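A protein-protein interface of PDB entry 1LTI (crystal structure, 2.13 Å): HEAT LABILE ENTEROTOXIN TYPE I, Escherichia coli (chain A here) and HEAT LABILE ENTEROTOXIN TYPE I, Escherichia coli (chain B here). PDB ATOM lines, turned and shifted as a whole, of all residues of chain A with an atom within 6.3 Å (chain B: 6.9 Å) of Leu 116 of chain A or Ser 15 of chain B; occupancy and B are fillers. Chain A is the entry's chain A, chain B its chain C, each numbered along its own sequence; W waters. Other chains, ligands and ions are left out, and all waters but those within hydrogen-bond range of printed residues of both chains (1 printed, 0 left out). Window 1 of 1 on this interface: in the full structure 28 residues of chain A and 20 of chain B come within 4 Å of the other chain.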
ATOM      1  N   PRO A  24      15.617  13.344 -19.864  1.00  0.00           N
ATOM      2  CA  PRO A  24      16.470  12.437 -19.094  1.00  0.00           C
ATOM      3  C   PRO A  24      17.183  11.539 -20.135  1.00  0.00           C
ATOM      4  O   PRO A  24      16.824  11.554 -21.327  1.00  0.00           O
ATOM      5  CB  PRO A  24      15.458  11.652 -18.254  1.00  0.00           C
ATOM      6  CG  PRO A  24      14.311  12.618 -18.111  1.00  0.00           C
ATOM      7  CD  PRO A  24      14.202  13.161 -19.505  1.00  0.00           C
ATOM      8  N   TYR A  30       9.901  14.865 -25.493  1.00  0.00           N
ATOM      9  CA  TYR A  30       9.268  14.912 -24.182  1.00  0.00           C
ATOM     10  C   TYR A  30       8.029  14.043 -24.068  1.00  0.00           C
ATOM     11  O   TYR A  30       7.909  13.274 -23.115  1.00  0.00           O
ATOM     12  CB  TYR A  30       8.925  16.342 -23.769  1.00  0.00           C
ATOM     13  CG  TYR A  30       8.290  16.442 -22.397  1.00  0.00           C
ATOM     14  CD1 TYR A  30       8.981  16.033 -21.252  1.00  0.00           C
ATOM     15  CD2 TYR A  30       7.001  16.960 -22.241  1.00  0.00           C
ATOM     16  CE1 TYR A  30       8.402  16.142 -19.980  1.00  0.00           C
ATOM     17  CE2 TYR A  30       6.408  17.075 -20.979  1.00  0.00           C
ATOM     18  CZ  TYR A  30       7.113  16.666 -19.850  1.00  0.00           C
ATOM     19  OH  TYR A  30       6.530  16.793 -18.614  1.00  0.00           O
ATOM     20  N   ILE A  39      11.681   4.357 -14.939  1.00  0.00           N
ATOM     21  CA  ILE A  39      11.574   5.570 -14.146  1.00  0.00           C
ATOM     22  C   ILE A  39      11.713   5.231 -12.661  1.00  0.00           C
ATOM     23  O   ILE A  39      10.763   4.756 -12.039  1.00  0.00           O
ATOM     24  CB  ILE A  39      10.218   6.273 -14.397  1.00  0.00           C
ATOM     25  CG1 ILE A  39       9.973   6.445 -15.901  1.00  0.00           C
ATOM     26  CG2 ILE A  39      10.219   7.636 -13.723  1.00  0.00           C
ATOM     27  CD1 ILE A  39       8.534   6.742 -16.267  1.00  0.00           C
ATOM     28  N   ASN A  40      12.887   5.504 -12.093  1.00  0.00           N
ATOM     29  CA  ASN A  40      13.155   5.198 -10.686  1.00  0.00           C
ATOM     30  C   ASN A  40      14.002   6.283 -10.025  1.00  0.00           C
ATOM     31  O   ASN A  40      15.113   6.569 -10.479  1.00  0.00           O
ATOM     32  CB  ASN A  40      13.900   3.860 -10.592  1.00  0.00           C
ATOM     33  CG  ASN A  40      14.002   3.337  -9.173  1.00  0.00           C
ATOM     34  OD1 ASN A  40      14.523   4.004  -8.263  1.00  0.00           O
ATOM     35  ND2 ASN A  40      13.518   2.125  -8.978  1.00  0.00           N
ATOM     36  N   LEU A  41      13.508   6.836  -8.921  1.00  0.00           N
ATOM     37  CA  LEU A  41      14.221   7.890  -8.209  1.00  0.00           C
ATOM     38  C   LEU A  41      15.513   7.422  -7.566  1.00  0.00           C
ATOM     39  O   LEU A  41      16.578   7.953  -7.879  1.00  0.00           O
ATOM     40  CB  LEU A  41      13.320   8.556  -7.157  1.00  0.00           C
ATOM     41  CG  LEU A  41      13.847   9.763  -6.362  1.00  0.00           C
ATOM     42  CD1 LEU A  41      14.213  10.882  -7.302  1.00  0.00           C
ATOM     43  CD2 LEU A  41      12.819  10.261  -5.349  1.00  0.00           C
ATOM     44  N   GLY A  58      14.815   8.152 -15.908  1.00  0.00           N
ATOM     45  CA  GLY A  58      13.620   8.981 -15.973  1.00  0.00           C
ATOM     46  C   GLY A  58      13.575  10.279 -15.187  1.00  0.00           C
ATOM     47  O   GLY A  58      12.497  10.855 -15.044  1.00  0.00           O
ATOM     48  N   TYR A  59      14.713  10.736 -14.672  1.00  0.00           N
ATOM     49  CA  TYR A  59      14.778  11.984 -13.918  1.00  0.00           C
ATOM     50  C   TYR A  59      15.945  12.876 -14.356  1.00  0.00           C
ATOM     51  O   TYR A  59      17.007  12.390 -14.752  1.00  0.00           O
ATOM     52  CB  TYR A  59      14.938  11.717 -12.426  1.00  0.00           C
ATOM     53  CG  TYR A  59      13.728  11.181 -11.698  1.00  0.00           C
ATOM     54  CD1 TYR A  59      13.392   9.825 -11.758  1.00  0.00           C
ATOM     55  CD2 TYR A  59      12.976  12.010 -10.878  1.00  0.00           C
ATOM     56  CE1 TYR A  59      12.338   9.312 -11.008  1.00  0.00           C
ATOM     57  CE2 TYR A  59      11.930  11.511 -10.125  1.00  0.00           C
ATOM     58  CZ  TYR A  59      11.614  10.165 -10.186  1.00  0.00           C
ATOM     59  OH  TYR A  59      10.604   9.686  -9.379  1.00  0.00           O
ATOM     60  N   VAL A  60      15.733  14.183 -14.279  1.00  0.00           N
ATOM     61  CA  VAL A  60      16.752  15.165 -14.614  1.00  0.00           C
ATOM     62  C   VAL A  60      16.919  15.941 -13.309  1.00  0.00           C
ATOM     63  O   VAL A  60      15.937  16.409 -12.738  1.00  0.00           O
ATOM     64  CB  VAL A  60      16.289  16.116 -15.762  1.00  0.00           C
ATOM     65  CG1 VAL A  60      17.255  17.266 -15.911  1.00  0.00           C
ATOM     66  CG2 VAL A  60      16.221  15.361 -17.086  1.00  0.00           C
ATOM     67  N   ASN A  93       6.194  18.504 -10.996  1.00  0.00           N
ATOM     68  CA  ASN A  93       6.924  17.366 -11.561  1.00  0.00           C
ATOM     69  C   ASN A  93       8.296  17.175 -10.901  1.00  0.00           C
ATOM     70  O   ASN A  93       9.006  16.208 -11.192  1.00  0.00           O
ATOM     71  CB  ASN A  93       7.083  17.481 -13.088  1.00  0.00           C
ATOM     72  CG  ASN A  93       7.902  18.698 -13.516  1.00  0.00           C
ATOM     73  OD1 ASN A  93       8.028  19.664 -12.771  1.00  0.00           O
ATOM     74  ND2 ASN A  93       8.459  18.650 -14.715  1.00  0.00           N
ATOM     75  N   MET A  94       8.654  18.070  -9.987  1.00  0.00           N
ATOM     76  CA  MET A  94       9.948  17.992  -9.327  1.00  0.00           C
ATOM     77  C   MET A  94       9.907  17.547  -7.880  1.00  0.00           C
ATOM     78  O   MET A  94       9.029  17.972  -7.130  1.00  0.00           O
ATOM     79  CB  MET A  94      10.663  19.323  -9.443  1.00  0.00           C
ATOM     80  CG  MET A  94      11.218  19.539 -10.819  1.00  0.00           C
ATOM     81  SD  MET A  94      11.566  21.232 -11.059  1.00  0.00           S
ATOM     82  CE  MET A  94      12.932  21.131 -12.205  1.00  0.00           C
ATOM     83  N   PHE A  95      10.884  16.711  -7.513  1.00  0.00           N
ATOM     84  CA  PHE A  95      11.031  16.144  -6.170  1.00  0.00           C
ATOM     85  C   PHE A  95      12.418  16.387  -5.567  1.00  0.00           C
ATOM     86  O   PHE A  95      13.449  16.211  -6.238  1.00  0.00           O
ATOM     87  CB  PHE A  95      10.763  14.630  -6.209  1.00  0.00           C
ATOM     88  CG  PHE A  95       9.310  14.264  -6.420  1.00  0.00           C
ATOM     89  CD1 PHE A  95       8.381  14.425  -5.387  1.00  0.00           C
ATOM     90  CD2 PHE A  95       8.877  13.749  -7.637  1.00  0.00           C
ATOM     91  CE1 PHE A  95       7.055  14.081  -5.558  1.00  0.00           C
ATOM     92  CE2 PHE A  95       7.550  13.401  -7.814  1.00  0.00           C
ATOM     93  CZ  PHE A  95       6.636  13.567  -6.770  1.00  0.00           C
ATOM     94  N   SER A 114      15.039  16.667  -8.416  1.00  0.00           N
ATOM     95  CA  SER A 114      14.849  16.050  -9.721  1.00  0.00           C
ATOM     96  C   SER A 114      13.453  16.126 -10.319  1.00  0.00           C
ATOM     97  O   SER A 114      12.460  15.836  -9.646  1.00  0.00           O
ATOM     98  CB  SER A 114      15.265  14.592  -9.662  1.00  0.00           C
ATOM     99  OG  SER A 114      16.654  14.479  -9.444  1.00  0.00           O
ATOM    100  N   ALA A 115      13.405  16.437 -11.612  1.00  0.00           N
ATOM    101  CA  ALA A 115      12.166  16.541 -12.373  1.00  0.00           C
ATOM    102  C   ALA A 115      11.859  15.188 -12.985  1.00  0.00           C
ATOM    103  O   ALA A 115      12.631  14.687 -13.811  1.00  0.00           O
ATOM    104  CB  ALA A 115      12.314  17.559 -13.466  1.00  0.00           C
ATOM    105  N   LEU A 116      10.750  14.588 -12.544  1.00  0.00           N
ATOM    106  CA  LEU A 116      10.307  13.287 -13.023  1.00  0.00           C
ATOM    107  C   LEU A 116       9.889  13.422 -14.470  1.00  0.00           C
ATOM    108  O   LEU A 116       9.032  14.240 -14.795  1.00  0.00           O
ATOM    109  CB  LEU A 116       9.140  12.792 -12.159  1.00  0.00           C
ATOM    110  CG  LEU A 116       8.097  11.755 -12.612  1.00  0.00           C
ATOM    111  CD1 LEU A 116       8.702  10.574 -13.319  1.00  0.00           C
ATOM    112  CD2 LEU A 116       7.349  11.285 -11.384  1.00  0.00           C
ATOM    113  N   GLY A 117      10.552  12.658 -15.332  1.00  0.00           N
ATOM    114  CA  GLY A 117      10.256  12.664 -16.757  1.00  0.00           C
ATOM    115  C   GLY A 117      10.893  13.746 -17.616  1.00  0.00           C
ATOM    116  O   GLY A 117      10.613  13.817 -18.818  1.00  0.00           O
ATOM    117  N   GLY A 118      11.741  14.573 -17.010  1.00  0.00           N
ATOM    118  CA  GLY A 118      12.405  15.639 -17.743  1.00  0.00           C
ATOM    119  C   GLY A 118      11.852  16.996 -17.352  1.00  0.00           C
ATOM    120  O   GLY A 118      11.143  17.115 -16.346  1.00  0.00           O
ATOM    121  N   ILE A 119      12.202  18.025 -18.128  1.00  0.00           N
ATOM    122  CA  ILE A 119      11.731  19.388 -17.878  1.00  0.00           C
ATOM    123  C   ILE A 119      11.187  19.968 -19.189  1.00  0.00           C
ATOM    124  O   ILE A 119      11.949  20.276 -20.100  1.00  0.00           O
ATOM    125  CB  ILE A 119      12.869  20.268 -17.336  1.00  0.00           C
ATOM    126  CG1 ILE A 119      13.486  19.582 -16.122  1.00  0.00           C
ATOM    127  CG2 ILE A 119      12.354  21.667 -16.995  1.00  0.00           C
ATOM    128  CD1 ILE A 119      14.566  20.338 -15.469  1.00  0.00           C
ATOM    129  N   ARG A 163       6.047   7.017  -2.320  1.00  0.00           N
ATOM    130  CA  ARG A 163       5.761   5.778  -3.031  1.00  0.00           C
ATOM    131  C   ARG A 163       6.562   5.666  -4.341  1.00  0.00           C
ATOM    132  O   ARG A 163       6.802   4.561  -4.859  1.00  0.00           O
ATOM    133  CB  ARG A 163       4.246   5.634  -3.278  1.00  0.00           C
ATOM    134  CG  ARG A 163       3.502   6.908  -3.669  1.00  0.00           C
ATOM    135  CD  ARG A 163       2.084   6.607  -4.179  1.00  0.00           C
ATOM    136  NE  ARG A 163       1.377   7.803  -4.669  1.00  0.00           N
ATOM    137  CZ  ARG A 163       1.698   8.498  -5.768  1.00  0.00           C
ATOM    138  NH1 ARG A 163       2.727   8.146  -6.534  1.00  0.00           N
ATOM    139  NH2 ARG A 163       0.968   9.549  -6.121  1.00  0.00           N
ATOM    140  N   LEU A 164       6.981   6.823  -4.859  1.00  0.00           N
ATOM    141  CA  LEU A 164       7.769   6.908  -6.092  1.00  0.00           C
ATOM    142  C   LEU A 164       9.264   6.776  -5.774  1.00  0.00           C
ATOM    143  O   LEU A 164      10.088   6.771  -6.687  1.00  0.00           O
ATOM    144  CB  LEU A 164       7.517   8.242  -6.815  1.00  0.00           C
ATOM    145  CG  LEU A 164       6.081   8.632  -7.176  1.00  0.00           C
ATOM    146  CD1 LEU A 164       6.081   9.799  -8.122  1.00  0.00           C
ATOM    147  CD2 LEU A 164       5.374   7.487  -7.834  1.00  0.00           C
ATOM    148  N   ALA A 165       9.590   6.604  -4.487  1.00  0.00           N
ATOM    149  CA  ALA A 165      10.970   6.483  -3.988  1.00  0.00           C
ATOM    150  C   ALA A 165      11.920   5.482  -4.652  1.00  0.00           C
ATOM    151  O   ALA A 165      13.130   5.522  -4.406  1.00  0.00           O
ATOM    152  CB  ALA A 165      10.965   6.269  -2.483  1.00  0.00           C
ATOM    153  N   GLU B  10       5.507  -1.813  -9.401  1.00  0.00           N
ATOM    154  CA  GLU B  10       4.707  -0.748  -8.824  1.00  0.00           C
ATOM    155  C   GLU B  10       5.311   0.625  -9.026  1.00  0.00           C
ATOM    156  O   GLU B  10       4.692   1.480  -9.669  1.00  0.00           O
ATOM    157  CB  GLU B  10       4.503  -0.997  -7.338  1.00  0.00           C
ATOM    158  CG  GLU B  10       3.402  -1.958  -7.078  1.00  0.00           C
ATOM    159  CD  GLU B  10       2.149  -1.527  -7.777  1.00  0.00           C
ATOM    160  OE1 GLU B  10       1.494  -0.585  -7.279  1.00  0.00           O
ATOM    161  OE2 GLU B  10       1.843  -2.103  -8.841  1.00  0.00           O
ATOM    162  N   THR B  11       6.502   0.839  -8.462  1.00  0.00           N
ATOM    163  CA  THR B  11       7.199   2.117  -8.589  1.00  0.00           C
ATOM    164  C   THR B  11       7.208   2.579 -10.048  1.00  0.00           C
ATOM    165  O   THR B  11       6.859   3.714 -10.352  1.00  0.00           O
ATOM    166  CB  THR B  11       8.650   2.040  -8.022  1.00  0.00           C
ATOM    167  OG1 THR B  11       8.607   2.010  -6.584  1.00  0.00           O
ATOM    168  CG2 THR B  11       9.481   3.248  -8.479  1.00  0.00           C
ATOM    169  N   GLN B  12       7.516   1.654 -10.943  1.00  0.00           N
ATOM    170  CA  GLN B  12       7.559   1.930 -12.368  1.00  0.00           C
ATOM    171  C   GLN B  12       6.185   2.374 -12.897  1.00  0.00           C
ATOM    172  O   GLN B  12       6.080   3.373 -13.620  1.00  0.00           O
ATOM    173  CB  GLN B  12       8.047   0.674 -13.097  1.00  0.00           C
ATOM    174  CG  GLN B  12       7.925   0.730 -14.600  1.00  0.00           C
ATOM    175  CD  GLN B  12       8.683   1.891 -15.192  1.00  0.00           C
ATOM    176  OE1 GLN B  12       9.751   2.263 -14.704  1.00  0.00           O
ATOM    177  NE2 GLN B  12       8.134   2.478 -16.245  1.00  0.00           N
ATOM    178  N   ASN B  13       5.134   1.652 -12.514  1.00  0.00           N
ATOM    179  CA  ASN B  13       3.789   1.977 -12.966  1.00  0.00           C
ATOM    180  C   ASN B  13       3.251   3.236 -12.288  1.00  0.00           C
ATOM    181  O   ASN B  13       2.472   3.973 -12.877  1.00  0.00           O
ATOM    182  CB  ASN B  13       2.848   0.800 -12.706  1.00  0.00           C
ATOM    183  CG  ASN B  13       1.662   0.767 -13.671  1.00  0.00           C
ATOM    184  OD1 ASN B  13       1.603  -0.072 -14.570  1.00  0.00           O
ATOM    185  ND2 ASN B  13       0.713   1.673 -13.483  1.00  0.00           N
ATOM    186  N   LEU B  14       3.664   3.473 -11.049  1.00  0.00           N
ATOM    187  CA  LEU B  14       3.231   4.647 -10.294  1.00  0.00           C
ATOM    188  C   LEU B  14       3.871   5.941 -10.815  1.00  0.00           C
ATOM    189  O   LEU B  14       3.232   7.004 -10.843  1.00  0.00           O
ATOM    190  CB  LEU B  14       3.566   4.489  -8.806  1.00  0.00           C
ATOM    191  CG  LEU B  14       2.570   3.735  -7.925  1.00  0.00           C
ATOM    192  CD1 LEU B  14       2.967   3.886  -6.456  1.00  0.00           C
ATOM    193  CD2 LEU B  14       1.157   4.270  -8.155  1.00  0.00           C
ATOM    194  N   SER B  15       5.155   5.843 -11.156  1.00  0.00           N
ATOM    195  CA  SER B  15       5.936   6.950 -11.682  1.00  0.00           C
ATOM    196  C   SER B  15       5.409   7.358 -13.070  1.00  0.00           C
ATOM    197  O   SER B  15       5.252   8.545 -13.372  1.00  0.00           O
ATOM    198  CB  SER B  15       7.415   6.547 -11.715  1.00  0.00           C
ATOM    199  OG  SER B  15       7.885   6.267 -10.399  1.00  0.00           O
ATOM    200  N   THR B  16       5.114   6.376 -13.906  1.00  0.00           N
ATOM    201  CA  THR B  16       4.563   6.641 -15.222  1.00  0.00           C
ATOM    202  C   THR B  16       3.198   7.342 -15.080  1.00  0.00           C
ATOM    203  O   THR B  16       2.883   8.263 -15.837  1.00  0.00           O
ATOM    204  CB  THR B  16       4.401   5.322 -15.985  1.00  0.00           C
ATOM    205  OG1 THR B  16       5.695   4.800 -16.306  1.00  0.00           O
ATOM    206  CG2 THR B  16       3.574   5.512 -17.245  1.00  0.00           C
ATOM    207  N   ILE B  17       2.403   6.905 -14.102  1.00  0.00           N
ATOM    208  CA  ILE B  17       1.077   7.484 -13.832  1.00  0.00           C
ATOM    209  C   ILE B  17       1.174   8.966 -13.483  1.00  0.00           C
ATOM    210  O   ILE B  17       0.401   9.766 -13.987  1.00  0.00           O
ATOM    211  CB  ILE B  17       0.343   6.757 -12.654  1.00  0.00           C
ATOM    212  CG1 ILE B  17      -0.446   5.554 -13.164  1.00  0.00           C
ATOM    213  CG2 ILE B  17      -0.606   7.701 -11.925  1.00  0.00           C
ATOM    214  CD1 ILE B  17      -1.117   4.773 -12.029  1.00  0.00           C
ATOM    215  N   TYR B  18       2.077   9.305 -12.571  1.00  0.00           N
ATOM    216  CA  TYR B  18       2.284  10.687 -12.157  1.00  0.00           C
ATOM    217  C   TYR B  18       2.706  11.532 -13.358  1.00  0.00           C
ATOM    218  O   TYR B  18       2.222  12.656 -13.543  1.00  0.00           O
ATOM    219  CB  TYR B  18       3.382  10.727 -11.106  1.00  0.00           C
ATOM    220  CG  TYR B  18       3.455  12.000 -10.304  1.00  0.00           C
ATOM    221  CD1 TYR B  18       4.210  13.093 -10.740  1.00  0.00           C
ATOM    222  CD2 TYR B  18       2.837  12.085  -9.065  1.00  0.00           C
ATOM    223  CE1 TYR B  18       4.349  14.233  -9.945  1.00  0.00           C
ATOM    224  CE2 TYR B  18       2.970  13.213  -8.261  1.00  0.00           C
ATOM    225  CZ  TYR B  18       3.726  14.279  -8.699  1.00  0.00           C
ATOM    226  OH  TYR B  18       3.888  15.366  -7.864  1.00  0.00           O
ATOM    227  N   LEU B  19       3.598  10.962 -14.176  1.00  0.00           N
ATOM    228  CA  LEU B  19       4.113  11.627 -15.370  1.00  0.00           C
ATOM    229  C   LEU B  19       3.042  11.918 -16.421  1.00  0.00           C
ATOM    230  O   LEU B  19       2.962  13.045 -16.894  1.00  0.00           O
ATOM    231  CB  LEU B  19       5.256  10.827 -15.995  1.00  0.00           C
ATOM    232  CG  LEU B  19       5.819  11.420 -17.301  1.00  0.00           C
ATOM    233  CD1 LEU B  19       6.467  12.788 -17.077  1.00  0.00           C
ATOM    234  CD2 LEU B  19       6.823  10.458 -17.906  1.00  0.00           C
ATOM    235  N   ARG B  20       2.252  10.913 -16.806  1.00  0.00           N
ATOM    236  CA  ARG B  20       1.184  11.098 -17.792  1.00  0.00           C
ATOM    237  C   ARG B  20       0.171  12.148 -17.351  1.00  0.00           C
ATOM    238  O   ARG B  20      -0.404  12.855 -18.179  1.00  0.00           O
ATOM    239  CB  ARG B  20       0.463   9.782 -18.074  1.00  0.00           C
ATOM    240  CG  ARG B  20       1.357   8.755 -18.688  1.00  0.00           C
ATOM    241  CD  ARG B  20       2.083   9.336 -19.879  1.00  0.00           C
ATOM    242  NE  ARG B  20       3.379   8.695 -20.081  1.00  0.00           N
ATOM    243  CZ  ARG B  20       3.538   7.484 -20.608  1.00  0.00           C
ATOM    244  NH1 ARG B  20       2.478   6.779 -20.996  1.00  0.00           N
ATOM    245  NH2 ARG B  20       4.758   6.966 -20.715  1.00  0.00           N
ATOM    246  N   TYR B  22       0.903  14.789 -15.392  1.00  0.00           N
ATOM    247  CA  TYR B  22       1.577  16.061 -15.591  1.00  0.00           C
ATOM    248  C   TYR B  22       1.585  16.457 -17.088  1.00  0.00           C
ATOM    249  O   TYR B  22       1.170  17.556 -17.455  1.00  0.00           O
ATOM    250  CB  TYR B  22       3.001  15.994 -15.008  1.00  0.00           C
ATOM    251  CG  TYR B  22       3.726  17.317 -15.049  1.00  0.00           C
ATOM    252  CD1 TYR B  22       3.334  18.365 -14.213  1.00  0.00           C
ATOM    253  CD2 TYR B  22       4.762  17.551 -15.956  1.00  0.00           C
ATOM    254  CE1 TYR B  22       3.947  19.610 -14.273  1.00  0.00           C
ATOM    255  CE2 TYR B  22       5.375  18.788 -16.025  1.00  0.00           C
ATOM    256  CZ  TYR B  22       4.963  19.815 -15.174  1.00  0.00           C
ATOM    257  OH  TYR B  22       5.591  21.044 -15.181  1.00  0.00           O
HETATM  258  O   HOH W   1      10.418   6.837  -9.415  1.00  0.00           O
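Tyr 30 of chain A touches Tyr 22 of chain B (OH to CD2, 3.3 Å).
Ile 39 of chain A touches Ser 15 of chain B.
Ile 39 of chain A touches Thr 16 of chain B.
Tyr 18 of chain B touches Phe 95 of chain A.
Tyr 18 of chain B touches Leu 116 of chain A.
CD1 of Leu 19 of chain B touches O of Leu 116 of chain A, 3.7 Å away.
CA of Gly 117 of chain A touches CD1 of Leu 19 of chain B, at 3.8 Å.
Arg 163 of chain A touches Thr 11 of chain B (O to OG1, 3.6 Å).
Leu 164 of chain A touches Thr 11 of chain B.
Leu 14 of chain B touches Leu 164 of chain A.
Water W1 lies within hydrogen-bond range of the backbone carbonyl oxygen of Leu 164 of chain A (2.7 Å), the side-chain hydroxyl of Ser 15 of chain B (2.8 Å), the side-chain hydroxyl of Tyr 59 of chain A (2.9 Å), the backbone NH of Leu 41 of chain A (3.1 Å) and the backbone carbonyl oxygen of Ile 39 of chain A (3.4 Å).
Printed residues of chain B within 4 Å of Leu 116 of chain A: Ser 15 (3.98 Å), Tyr 18 (3.7 Å) and Leu 19 (3.7 Å).
Printed residues of chain A within 4 Å of Ser 15 of chain B: Ile 39 (3.6 Å), Leu 116 (3.98 Å) and Leu 164 (3.7 Å).
Printed residues of chain A within 4 Å of Tyr 18 of chain B: Phe 95 (3.5 Å) and Leu 116 (3.7 Å).
Printed residues of chain A within 4 Å of Tyr 22 of chain B: Tyr 30 and Asn 93.
Of the printed residues of chain B, Arg 163 of chain A touches Thr 11 (3.6 Å) and Leu 14 (3.7 Å).
Met 94 of chain A touches none of the printed residues of chain B.
Tyr 59 of chain A touches none of the printed residues of chain B.
The nearest printed residue of chain B that does not touch Leu 116 of chain A is Tyr 22 of chain B (5.5 Å).
The nearest printed residue of chain A that does not touch Ser 15 of chain B is Tyr 59 of chain A (4.5 Å).
The backbone NH of Ile 39 of chain A lies within hydrogen-bond range of the side-chain amide oxygen of Gln 12 of chain B.
Of the 20 printed residues of chain A, 8 touch a printed residue of chain B.
Printed residues of chain A that touch a printed residue of chain B: Tyr 30, Ile 39, Asn 93, Phe 95, Leu 116, Gly 117, Arg 163 and Leu 164.
Hydrophobic or aromatic side chains of chain A that line the printed part of chain B: Tyr 30, Ile 39, Phe 95, Leu 116 and Leu 164.
Along chain A the printed residues that touch a printed residue of chain B span positions 30 to 164.
Of the 12 printed residues of chain B, 8 touch a printed residue of chain A.
Among the printed residues, 15 pairs touch across the chains.
Among the printed residues, no Asp or Glu carboxylate lies within 4 Å of a Lys or Arg side-chain nitrogen of the other chain.
The backbone carbonyl oxygen (O) of Gln 12 of chain B is in hydrogen-bond range of the side-chain hydroxyl (OG1) of Thr 16 of chain B, 3.1 Å away.
O of Phe 95 of chain A sits at hydrogen-bond distance from N of Ser 114 of chain A.
ND2 of Asn 93 of chain A sits at hydrogen-bond distance from O of Gly 118 of chain A, at 3.5 Å.
The backbone carbonyl oxygen (O) of Asn 93 of chain A sits at hydrogen-bond distance from the backbone NH (N) of Leu 116 of chain A (2.7 Å).
O of Thr 11 of chain B lies within hydrogen-bond range of OG of Ser 15 of chain B, at 2.8 Å.
N of Gly 117 of chain A sits at hydrogen-bond distance from O of Gly 58 of chain A.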
